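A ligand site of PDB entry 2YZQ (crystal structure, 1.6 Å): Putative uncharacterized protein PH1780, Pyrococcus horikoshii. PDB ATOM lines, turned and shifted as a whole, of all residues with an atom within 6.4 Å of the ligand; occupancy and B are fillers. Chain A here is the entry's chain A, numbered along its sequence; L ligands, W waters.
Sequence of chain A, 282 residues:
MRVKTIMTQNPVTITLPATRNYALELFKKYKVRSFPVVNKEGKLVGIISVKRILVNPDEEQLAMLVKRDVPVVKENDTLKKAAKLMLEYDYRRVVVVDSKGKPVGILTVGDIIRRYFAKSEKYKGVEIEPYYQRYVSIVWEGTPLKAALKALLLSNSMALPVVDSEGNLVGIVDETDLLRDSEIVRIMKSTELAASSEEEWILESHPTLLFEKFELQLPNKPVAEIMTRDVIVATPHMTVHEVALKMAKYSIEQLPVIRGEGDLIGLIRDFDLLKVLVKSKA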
ATOM      1  N   MET A 158      -9.761 -13.184   6.407  1.00  0.00           N
ATOM      2  CA  MET A 158     -11.105 -13.107   6.969  1.00  0.00           C
ATOM      3  C   MET A 158     -11.051 -13.003   8.492  1.00  0.00           C
ATOM      4  O   MET A 158     -12.057 -12.692   9.126  1.00  0.00           O
ATOM      5  CB  MET A 158     -11.913 -14.331   6.561  1.00  0.00           C
ATOM      6  CG  MET A 158     -12.156 -14.429   5.076  1.00  0.00           C
ATOM      7  SD  MET A 158     -13.227 -15.816   4.700  1.00  0.00           S
ATOM      8  CE  MET A 158     -14.769 -15.224   5.349  1.00  0.00           C
ATOM      9  N   ALA A 159      -9.880 -13.248   9.065  1.00  0.00           N
ATOM     10  CA  ALA A 159      -9.749 -13.191  10.515  1.00  0.00           C
ATOM     11  C   ALA A 159      -8.488 -12.494  10.988  1.00  0.00           C
ATOM     12  O   ALA A 159      -7.477 -12.450  10.283  1.00  0.00           O
ATOM     13  CB  ALA A 159      -9.792 -14.602  11.102  1.00  0.00           C
ATOM     14  N   ILE A 172      -8.377 -15.345  18.288  1.00  0.00           N
ATOM     15  CA  ILE A 172      -8.568 -15.017  16.882  1.00  0.00           C
ATOM     16  C   ILE A 172     -10.007 -14.531  16.759  1.00  0.00           C
ATOM     17  O   ILE A 172     -10.869 -14.938  17.531  1.00  0.00           O
ATOM     18  CB  ILE A 172      -8.292 -16.272  15.997  1.00  0.00           C
ATOM     19  CG1 ILE A 172      -8.330 -15.888  14.524  1.00  0.00           C
ATOM     20  CG2 ILE A 172      -9.274 -17.388  16.343  1.00  0.00           C
ATOM     21  CD1 ILE A 172      -7.553 -16.845  13.644  1.00  0.00           C
ATOM     22  N   VAL A 173     -10.263 -13.636  15.801  1.00  0.00           N
ATOM     23  CA  VAL A 173     -11.612 -13.103  15.652  1.00  0.00           C
ATOM     24  C   VAL A 173     -11.970 -12.796  14.201  1.00  0.00           C
ATOM     25  O   VAL A 173     -11.106 -12.392  13.420  1.00  0.00           O
ATOM     26  CB  VAL A 173     -11.776 -11.795  16.484  1.00  0.00           C
ATOM     27  CG1 VAL A 173     -10.829 -10.704  15.964  1.00  0.00           C
ATOM     28  CG2 VAL A 173     -13.214 -11.323  16.441  1.00  0.00           C
ATOM     29  N   ASP A 174     -13.232 -13.028  13.836  1.00  0.00           N
ATOM     30  CA  ASP A 174     -13.693 -12.722  12.490  1.00  0.00           C
ATOM     31  C   ASP A 174     -15.081 -12.084  12.546  1.00  0.00           C
ATOM     32  O   ASP A 174     -15.625 -11.875  13.630  1.00  0.00           O
ATOM     33  CB  ASP A 174     -13.657 -13.948  11.558  1.00  0.00           C
ATOM     34  CG  ASP A 174     -14.797 -14.931  11.779  1.00  0.00           C
ATOM     35  OD1 ASP A 174     -15.662 -14.722  12.643  1.00  0.00           O
ATOM     36  OD2 ASP A 174     -14.808 -15.949  11.048  1.00  0.00           O
ATOM     37  N   GLU A 175     -15.618 -11.751  11.378  1.00  0.00           N
ATOM     38  CA  GLU A 175     -16.911 -11.085  11.286  1.00  0.00           C
ATOM     39  C   GLU A 175     -18.047 -11.798  12.025  1.00  0.00           C
ATOM     40  O   GLU A 175     -18.849 -11.155  12.688  1.00  0.00           O
ATOM     41  CB  GLU A 175     -17.265 -10.895   9.809  1.00  0.00           C
ATOM     42  CG  GLU A 175     -18.566 -10.166   9.544  1.00  0.00           C
ATOM     43  CD  GLU A 175     -18.751  -9.901   8.063  1.00  0.00           C
ATOM     44  OE1 GLU A 175     -18.478 -10.809   7.248  1.00  0.00           O
ATOM     45  OE2 GLU A 175     -19.189  -8.775   7.709  1.00  0.00           O
ATOM     46  N   THR A 176     -18.086 -13.113  11.924  1.00  0.00           N
ATOM     47  CA  THR A 176     -19.151 -13.874  12.578  1.00  0.00           C
ATOM     48  C   THR A 176     -19.135 -13.755  14.098  1.00  0.00           C
ATOM     49  O   THR A 176     -20.166 -13.945  14.758  1.00  0.00           O
ATOM     50  CB  THR A 176     -19.088 -15.378  12.206  1.00  0.00           C
ATOM     51  OG1 THR A 176     -17.988 -15.998  12.894  1.00  0.00           O
ATOM     52  CG2 THR A 176     -18.903 -15.539  10.706  1.00  0.00           C
ATOM     53  N   ASP A 177     -17.981 -13.421  14.673  1.00  0.00           N
ATOM     54  CA  ASP A 177     -17.882 -13.299  16.115  1.00  0.00           C
ATOM     55  C   ASP A 177     -18.613 -12.073  16.661  1.00  0.00           C
ATOM     56  O   ASP A 177     -18.878 -11.983  17.851  1.00  0.00           O
ATOM     57  CB  ASP A 177     -16.410 -13.265  16.553  1.00  0.00           C
ATOM     58  CG  ASP A 177     -15.709 -14.578  16.299  1.00  0.00           C
ATOM     59  OD1 ASP A 177     -16.360 -15.631  16.480  1.00  0.00           O
ATOM     60  OD2 ASP A 177     -14.518 -14.572  15.931  1.00  0.00           O
ATOM     61  N   ARG A 180     -21.628 -12.502  18.768  1.00  0.00           N
ATOM     62  CA  ARG A 180     -21.483 -12.972  20.143  1.00  0.00           C
ATOM     63  C   ARG A 180     -21.751 -11.825  21.098  1.00  0.00           C
ATOM     64  O   ARG A 180     -21.807 -12.022  22.315  1.00  0.00           O
ATOM     65  CB  ARG A 180     -20.072 -13.519  20.387  1.00  0.00           C
ATOM     66  CG  ARG A 180     -19.796 -14.867  19.769  1.00  0.00           C
ATOM     67  CD  ARG A 180     -18.316 -15.190  19.860  1.00  0.00           C
ATOM     68  NE  ARG A 180     -18.002 -16.531  19.390  1.00  0.00           N
ATOM     69  CZ  ARG A 180     -16.757 -16.973  19.224  1.00  0.00           C
ATOM     70  NH1 ARG A 180     -15.732 -16.178  19.478  1.00  0.00           N
ATOM     71  NH2 ARG A 180     -16.551 -18.216  18.804  1.00  0.00           N
ATOM     72  N   ILE A 226     -15.244 -10.915  22.503  1.00  0.00           N
ATOM     73  CA  ILE A 226     -15.934 -11.728  21.495  1.00  0.00           C
ATOM     74  C   ILE A 226     -14.996 -12.665  20.745  1.00  0.00           C
ATOM     75  O   ILE A 226     -15.428 -13.398  19.861  1.00  0.00           O
ATOM     76  CB  ILE A 226     -16.652 -10.859  20.443  1.00  0.00           C
ATOM     77  CG1 ILE A 226     -15.638 -10.033  19.648  1.00  0.00           C
ATOM     78  CG2 ILE A 226     -17.674  -9.948  21.127  1.00  0.00           C
ATOM     79  CD1 ILE A 226     -16.213  -9.385  18.400  1.00  0.00           C
ATOM     80  N   MET A 227     -13.720 -12.689  21.121  1.00  0.00           N
ATOM     81  CA  MET A 227     -12.766 -13.522  20.417  1.00  0.00           C
ATOM     82  C   MET A 227     -12.828 -15.012  20.766  1.00  0.00           C
ATOM     83  O   MET A 227     -13.323 -15.413  21.821  1.00  0.00           O
ATOM     84  CB  MET A 227     -11.336 -13.019  20.671  1.00  0.00           C
ATOM     85  CG  MET A 227     -10.806 -13.342  22.061  1.00  0.00           C
ATOM     86  SD  MET A 227      -9.127 -12.727  22.275  1.00  0.00           S
ATOM     87  CE  MET A 227      -8.726 -13.362  23.908  1.00  0.00           C
ATOM     88  N   THR A 228     -12.330 -15.827  19.835  1.00  0.00           N
ATOM     89  CA  THR A 228     -12.256 -17.276  20.021  1.00  0.00           C
ATOM     90  C   THR A 228     -10.889 -17.502  20.679  1.00  0.00           C
ATOM     91  O   THR A 228      -9.856 -17.125  20.120  1.00  0.00           O
ATOM     92  CB  THR A 228     -12.312 -18.001  18.666  1.00  0.00           C
ATOM     93  OG1 THR A 228     -13.595 -17.775  18.050  1.00  0.00           O
ATOM     94  CG2 THR A 228     -12.075 -19.492  18.851  1.00  0.00           C
ATOM     95  N   ASP A 230      -9.490 -20.619  21.732  1.00  0.00           N
ATOM     96  CA  ASP A 230      -8.774 -21.821  21.315  1.00  0.00           C
ATOM     97  C   ASP A 230      -8.468 -21.718  19.834  1.00  0.00           C
ATOM     98  O   ASP A 230      -9.311 -22.026  18.993  1.00  0.00           O
ATOM     99  CB  ASP A 230      -9.604 -23.076  21.604  1.00  0.00           C
ATOM    100  CG  ASP A 230      -8.855 -24.347  21.282  1.00  0.00           C
ATOM    101  OD1 ASP A 230      -7.613 -24.359  21.452  1.00  0.00           O
ATOM    102  OD2 ASP A 230      -9.492 -25.341  20.876  1.00  0.00           O
ATOM    103  N   VAL A 231      -7.254 -21.289  19.530  1.00  0.00           N
ATOM    104  CA  VAL A 231      -6.842 -21.096  18.144  1.00  0.00           C
ATOM    105  C   VAL A 231      -6.242 -22.345  17.509  1.00  0.00           C
ATOM    106  O   VAL A 231      -5.370 -23.011  18.080  1.00  0.00           O
ATOM    107  CB  VAL A 231      -5.803 -19.945  18.048  1.00  0.00           C
ATOM    108  CG1 VAL A 231      -5.621 -19.533  16.599  1.00  0.00           C
ATOM    109  CG2 VAL A 231      -6.272 -18.757  18.886  1.00  0.00           C
ATOM    110  N   ILE A 232      -6.760 -22.673  16.321  1.00  0.00           N
ATOM    111  CA  ILE A 232      -6.281 -23.816  15.558  1.00  0.00           C
ATOM    112  C   ILE A 232      -5.110 -23.275  14.753  1.00  0.00           C
ATOM    113  O   ILE A 232      -5.278 -22.387  13.916  1.00  0.00           O
ATOM    114  CB  ILE A 232      -7.364 -24.321  14.591  1.00  0.00           C
ATOM    115  CG1 ILE A 232      -8.641 -24.660  15.379  1.00  0.00           C
ATOM    116  CG2 ILE A 232      -6.847 -25.524  13.823  1.00  0.00           C
ATOM    117  CD1 ILE A 232      -8.419 -25.672  16.486  1.00  0.00           C
ATOM    118  N   VAL A 233      -3.923 -23.819  15.006  1.00  0.00           N
ATOM    119  CA  VAL A 233      -2.703 -23.340  14.352  1.00  0.00           C
ATOM    120  C   VAL A 233      -1.996 -24.305  13.413  1.00  0.00           C
ATOM    121  O   VAL A 233      -2.279 -25.506  13.388  1.00  0.00           O
ATOM    122  CB  VAL A 233      -1.649 -22.889  15.415  1.00  0.00           C
ATOM    123  CG1 VAL A 233      -2.243 -21.844  16.323  1.00  0.00           C
ATOM    124  CG2 VAL A 233      -1.191 -24.092  16.242  1.00  0.00           C
ATOM    125  N   TYR A 250     -13.010 -27.530  10.851  1.00  0.00           N
ATOM    126  CA  TYR A 250     -13.458 -26.411  11.662  1.00  0.00           C
ATOM    127  C   TYR A 250     -14.174 -25.317  10.872  1.00  0.00           C
ATOM    128  O   TYR A 250     -14.640 -24.331  11.453  1.00  0.00           O
ATOM    129  CB  TYR A 250     -12.272 -25.820  12.410  1.00  0.00           C
ATOM    130  CG  TYR A 250     -11.578 -26.811  13.324  1.00  0.00           C
ATOM    131  CD1 TYR A 250     -12.191 -27.234  14.508  1.00  0.00           C
ATOM    132  CD2 TYR A 250     -10.331 -27.343  13.004  1.00  0.00           C
ATOM    133  CE1 TYR A 250     -11.569 -28.159  15.339  1.00  0.00           C
ATOM    134  CE2 TYR A 250      -9.703 -28.263  13.824  1.00  0.00           C
ATOM    135  CZ  TYR A 250     -10.331 -28.671  15.000  1.00  0.00           C
ATOM    136  OH  TYR A 250      -9.699 -29.582  15.818  1.00  0.00           O
ATOM    137  N   SER A 251     -14.268 -25.491   9.556  1.00  0.00           N
ATOM    138  CA  SER A 251     -14.912 -24.511   8.680  1.00  0.00           C
ATOM    139  C   SER A 251     -14.273 -23.144   8.848  1.00  0.00           C
ATOM    140  O   SER A 251     -14.971 -22.144   9.032  1.00  0.00           O
ATOM    141  CB  SER A 251     -16.414 -24.435   8.966  1.00  0.00           C
ATOM    142  OG  SER A 251     -17.068 -25.638   8.579  1.00  0.00           O
ATOM    143  N   ILE A 252     -12.956 -23.108   8.783  1.00  0.00           N
ATOM    144  CA  ILE A 252     -12.209 -21.856   8.917  1.00  0.00           C
ATOM    145  C   ILE A 252     -11.359 -21.662   7.671  1.00  0.00           C
ATOM    146  O   ILE A 252     -10.877 -22.614   7.072  1.00  0.00           O
ATOM    147  CB  ILE A 252     -11.328 -21.875  10.177  1.00  0.00           C
ATOM    148  CG1 ILE A 252     -10.460 -23.140  10.185  1.00  0.00           C
ATOM    149  CG2 ILE A 252     -12.203 -21.795  11.425  1.00  0.00           C
ATOM    150  CD1 ILE A 252      -9.636 -23.319  11.461  1.00  0.00           C
ATOM    151  N   GLU A 253     -11.170 -20.393   7.295  1.00  0.00           N
ATOM    152  CA  GLU A 253     -10.413 -20.064   6.090  1.00  0.00           C
ATOM    153  C   GLU A 253      -8.940 -19.739   6.315  1.00  0.00           C
ATOM    154  O   GLU A 253      -8.218 -19.449   5.362  1.00  0.00           O
ATOM    155  CB  GLU A 253     -11.076 -18.886   5.383  1.00  0.00           C
ATOM    156  CG  GLU A 253     -12.515 -19.157   4.922  1.00  0.00           C
ATOM    157  CD  GLU A 253     -13.568 -18.809   5.975  1.00  0.00           C
ATOM    158  OE1 GLU A 253     -13.226 -18.653   7.164  1.00  0.00           O
ATOM    159  OE2 GLU A 253     -14.751 -18.703   5.596  1.00  0.00           O
ATOM    160  N   GLN A 254      -8.477 -19.791   7.569  1.00  0.00           N
ATOM    161  CA  GLN A 254      -7.089 -19.464   7.848  1.00  0.00           C
ATOM    162  C   GLN A 254      -6.596 -19.992   9.188  1.00  0.00           C
ATOM    163  O   GLN A 254      -7.343 -20.059  10.159  1.00  0.00           O
ATOM    164  CB  GLN A 254      -6.879 -17.947   7.829  1.00  0.00           C
ATOM    165  CG  GLN A 254      -7.646 -17.208   8.923  1.00  0.00           C
ATOM    166  CD  GLN A 254      -9.142 -17.215   8.708  1.00  0.00           C
ATOM    167  OE1 GLN A 254      -9.631 -16.749   7.680  1.00  0.00           O
ATOM    168  NE2 GLN A 254      -9.889 -17.731   9.684  1.00  0.00           N
ATOM    169  N   LEU A 255      -5.309 -20.349   9.231  1.00  0.00           N
ATOM    170  CA  LEU A 255      -4.683 -20.824  10.458  1.00  0.00           C
ATOM    171  C   LEU A 255      -3.423 -20.028  10.737  1.00  0.00           C
ATOM    172  O   LEU A 255      -2.557 -19.899   9.861  1.00  0.00           O
ATOM    173  CB  LEU A 255      -4.263 -22.298  10.358  1.00  0.00           C
ATOM    174  CG  LEU A 255      -5.292 -23.433  10.441  1.00  0.00           C
ATOM    175  CD1 LEU A 255      -6.232 -23.373   9.261  1.00  0.00           C
ATOM    176  CD2 LEU A 255      -4.552 -24.763  10.471  1.00  0.00           C
ATOM    177  N   PRO A 256      -3.315 -19.447  11.935  1.00  0.00           N
ATOM    178  CA  PRO A 256      -2.093 -18.688  12.228  1.00  0.00           C
ATOM    179  C   PRO A 256      -0.928 -19.692  12.160  1.00  0.00           C
ATOM    180  O   PRO A 256      -1.083 -20.855  12.531  1.00  0.00           O
ATOM    181  CB  PRO A 256      -2.331 -18.215  13.657  1.00  0.00           C
ATOM    182  CG  PRO A 256      -3.807 -17.967  13.677  1.00  0.00           C
ATOM    183  CD  PRO A 256      -4.358 -19.172  12.928  1.00  0.00           C
HETATM  184  N1  LIG L   1     -16.659 -17.271   6.789  1.00  0.00           N
HETATM  185  C1  LIG L   1     -17.277 -18.298   7.628  1.00  0.00           C
HETATM  186  C2  LIG L   1     -18.727 -17.937   7.899  1.00  0.00           C
HETATM  187  O1  LIG L   1     -19.492 -18.775   8.349  1.00  0.00           O
HETATM  188  O2  LIG L   1     -19.131 -16.808   7.671  1.00  0.00           O
HETATM  189  C3  LIG L   1     -16.499 -18.406   8.945  1.00  0.00           C
HETATM  190  C4  LIG L   1     -16.796 -19.751   9.621  1.00  0.00           C
HETATM  191  S1  LIG L   1     -15.674 -20.010  11.018  1.00  0.00           S
HETATM  192  C5  LIG L   1     -16.451 -21.495  11.740  1.00  0.00           C
HETATM  193  C6  LIG L   1     -16.046 -18.674  12.188  1.00  0.00           C
HETATM  194  C7  LIG L   1     -15.466 -19.032  13.559  1.00  0.00           C
HETATM  195  O3  LIG L   1     -14.171 -19.657  13.400  1.00  0.00           O
HETATM  196  C8  LIG L   1     -15.265 -17.781  14.434  1.00  0.00           C
HETATM  197  O4  LIG L   1     -15.708 -18.062  15.766  1.00  0.00           O
HETATM  198  C9  LIG L   1     -13.750 -17.552  14.355  1.00  0.00           C
HETATM  199  O5  LIG L   1     -13.265 -16.827  15.492  1.00  0.00           O
HETATM  200  C10 LIG L   1     -13.243 -19.001  14.280  1.00  0.00           C
HETATM  201  N2  LIG L   1     -11.901 -19.125  13.744  1.00  0.00           N
HETATM  202  C11 LIG L   1     -11.377 -18.574  12.582  1.00  0.00           C
HETATM  203  N3  LIG L   1     -10.171 -19.028  12.389  1.00  0.00           N
HETATM  204  C12 LIG L   1      -9.801 -19.777  13.468  1.00  0.00           C
HETATM  205  C13 LIG L   1      -8.626 -20.453  13.890  1.00  0.00           C
HETATM  206  N4  LIG L   1      -7.472 -20.413  13.125  1.00  0.00           N
HETATM  207  N5  LIG L   1      -8.636 -21.132  15.047  1.00  0.00           N
HETATM  208  C14 LIG L   1      -9.716 -21.150  15.845  1.00  0.00           C
HETATM  209  N6  LIG L   1     -10.850 -20.566  15.474  1.00  0.00           N
HETATM  210  C15 LIG L   1     -10.921 -19.853  14.329  1.00  0.00           C
HETATM  211  O   HOH W   1     -12.881 -17.637   9.727  1.00  0.00           O
HETATM  212  O   HOH W   2     -18.728 -16.963  15.346  1.00  0.00           O
HETATM  213  O   HOH W   3     -14.712 -22.721  14.260  1.00  0.00           O
HETATM  214  O   HOH W   4     -22.076 -20.802   9.007  1.00  0.00           O
HETATM  215  O   HOH W   5     -22.196 -18.123   8.833  1.00  0.00           O
HETATM  216  O   HOH W   6     -15.345 -20.668  16.829  1.00  0.00           O
HETATM  217  O   HOH W   7     -17.384 -22.954  14.390  1.00  0.00           O
HETATM  218  O   HOH W   8     -15.635 -15.097   8.517  1.00  0.00           O
HETATM  219  O   HOH W   9     -13.064 -22.189  16.232  1.00  0.00           O
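OD1 of Asp 177 sits at hydrogen-bond distance from O4 of the ligand (2.6 Å). OE2 of Glu 253 lies within salt-bridge range of N1 of the ligand, at 2.7 Å. N5 of the ligand is in hydrogen-bond range of N of Ile 232, at 2.7 Å. The backbone carbonyl oxygen (O) of Ile 232 lies within hydrogen-bond range of a nitrogen (N4) of the ligand (3.1 Å). An oxygen (O5) of the ligand is in hydrogen-bond range of the side-chain hydroxyl (OG1) of Thr 228, at 2.7 Å. O of Gln 254 lies within hydrogen-bond range of N4 of the ligand (3.0 Å). A nitrogen (N3) of the ligand sits at hydrogen-bond distance from the side-chain amide nitrogen (NE2) of Gln 254 (3.0 Å). O4 of the ligand lies within hydrogen-bond range of NH2 of Arg 180 (3.2 Å).
OD1 of Asp 177 lies within salt-bridge range of NH1 of Arg 180. The side-chain carboxylate of Asp 177 lies within hydrogen-bond range of the backbone NH of Asp 174 (2.9 Å). The guanidinium group (NH1) of Arg 180 is in hydrogen-bond range of the side-chain hydroxyl (OG1) of Thr 228 (3.0 Å). N of Thr 228 is in hydrogen-bond range of O of Ile 172, 2.9 Å away. The guanidinium group (NH1) of Arg 180 sits close to the backbone carbonyl oxygen (O) of Met 227. NH1 of Arg 180 sits at hydrogen-bond distance from O of Ile 226, 2.8 Å away. OD1 of Asp 174 is in hydrogen-bond range of OG1 of Thr 176, 2.7 Å away.
A sulfur (S1) of the ligand lies close to the backbone carbonyl oxygen (O) of Ser 251. Met 158 touches the ligand (CE to N1, 3.1 Å). CG2 of Ile 172 touches C15 of the ligand (3.6 Å). Asp 174 touches the ligand (OD2 to C6, 3.2 Å). CG2 of Thr 176 touches O2 of the ligand (3.3 Å). Asp 230 touches the ligand (O to C14, 3.3 Å). Val 231 touches the ligand (CA to N5, 3.6 Å). Tyr 250 touches the ligand (O to C5, 3.4 Å). CG2 of Ile 252 touches O3 of the ligand (3.5 Å). Leu 255 touches the ligand. CD of Pro 256 touches N4 of the ligand, 3.4 Å away. 17 residues have an atom within 4 Å of the ligand: Met 158, Ile 172, Asp 174, Thr 176, Asp 177, Arg 180, Thr 228, Asp 230, Val 231, Ile 232, Tyr 250, Ser 251, Ile 252, Glu 253, Gln 254, Leu 255 and Pro 256. The nearest printed residue that does not touch the ligand is Val 173 (4.1 Å).
Water W6 lies within hydrogen-bond range of an oxygen (O4) of the ligand and the guanidinium group (NH2) of Arg 180. Water W8 lies within hydrogen-bond range of the side-chain carboxylate of Asp 174 and a nitrogen (N1) of the ligand. Water W3 lies within hydrogen-bond range of an oxygen (O3) of the ligand (3.2 Å) and the backbone carbonyl oxygen (O) of Tyr 250 (3.2 Å). Water W2 lies within hydrogen-bond range of the side-chain hydroxyl of Thr 176, the side-chain carboxylate of Asp 177 and an oxygen (O4) of the ligand. Water W1 lies within hydrogen-bond range of the side-chain carboxylate of Glu 253 (2.8 Å), the side-chain carboxylate of Asp 174 (2.9 Å) and the side-chain amide nitrogen of Gln 254 (3.0 Å).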
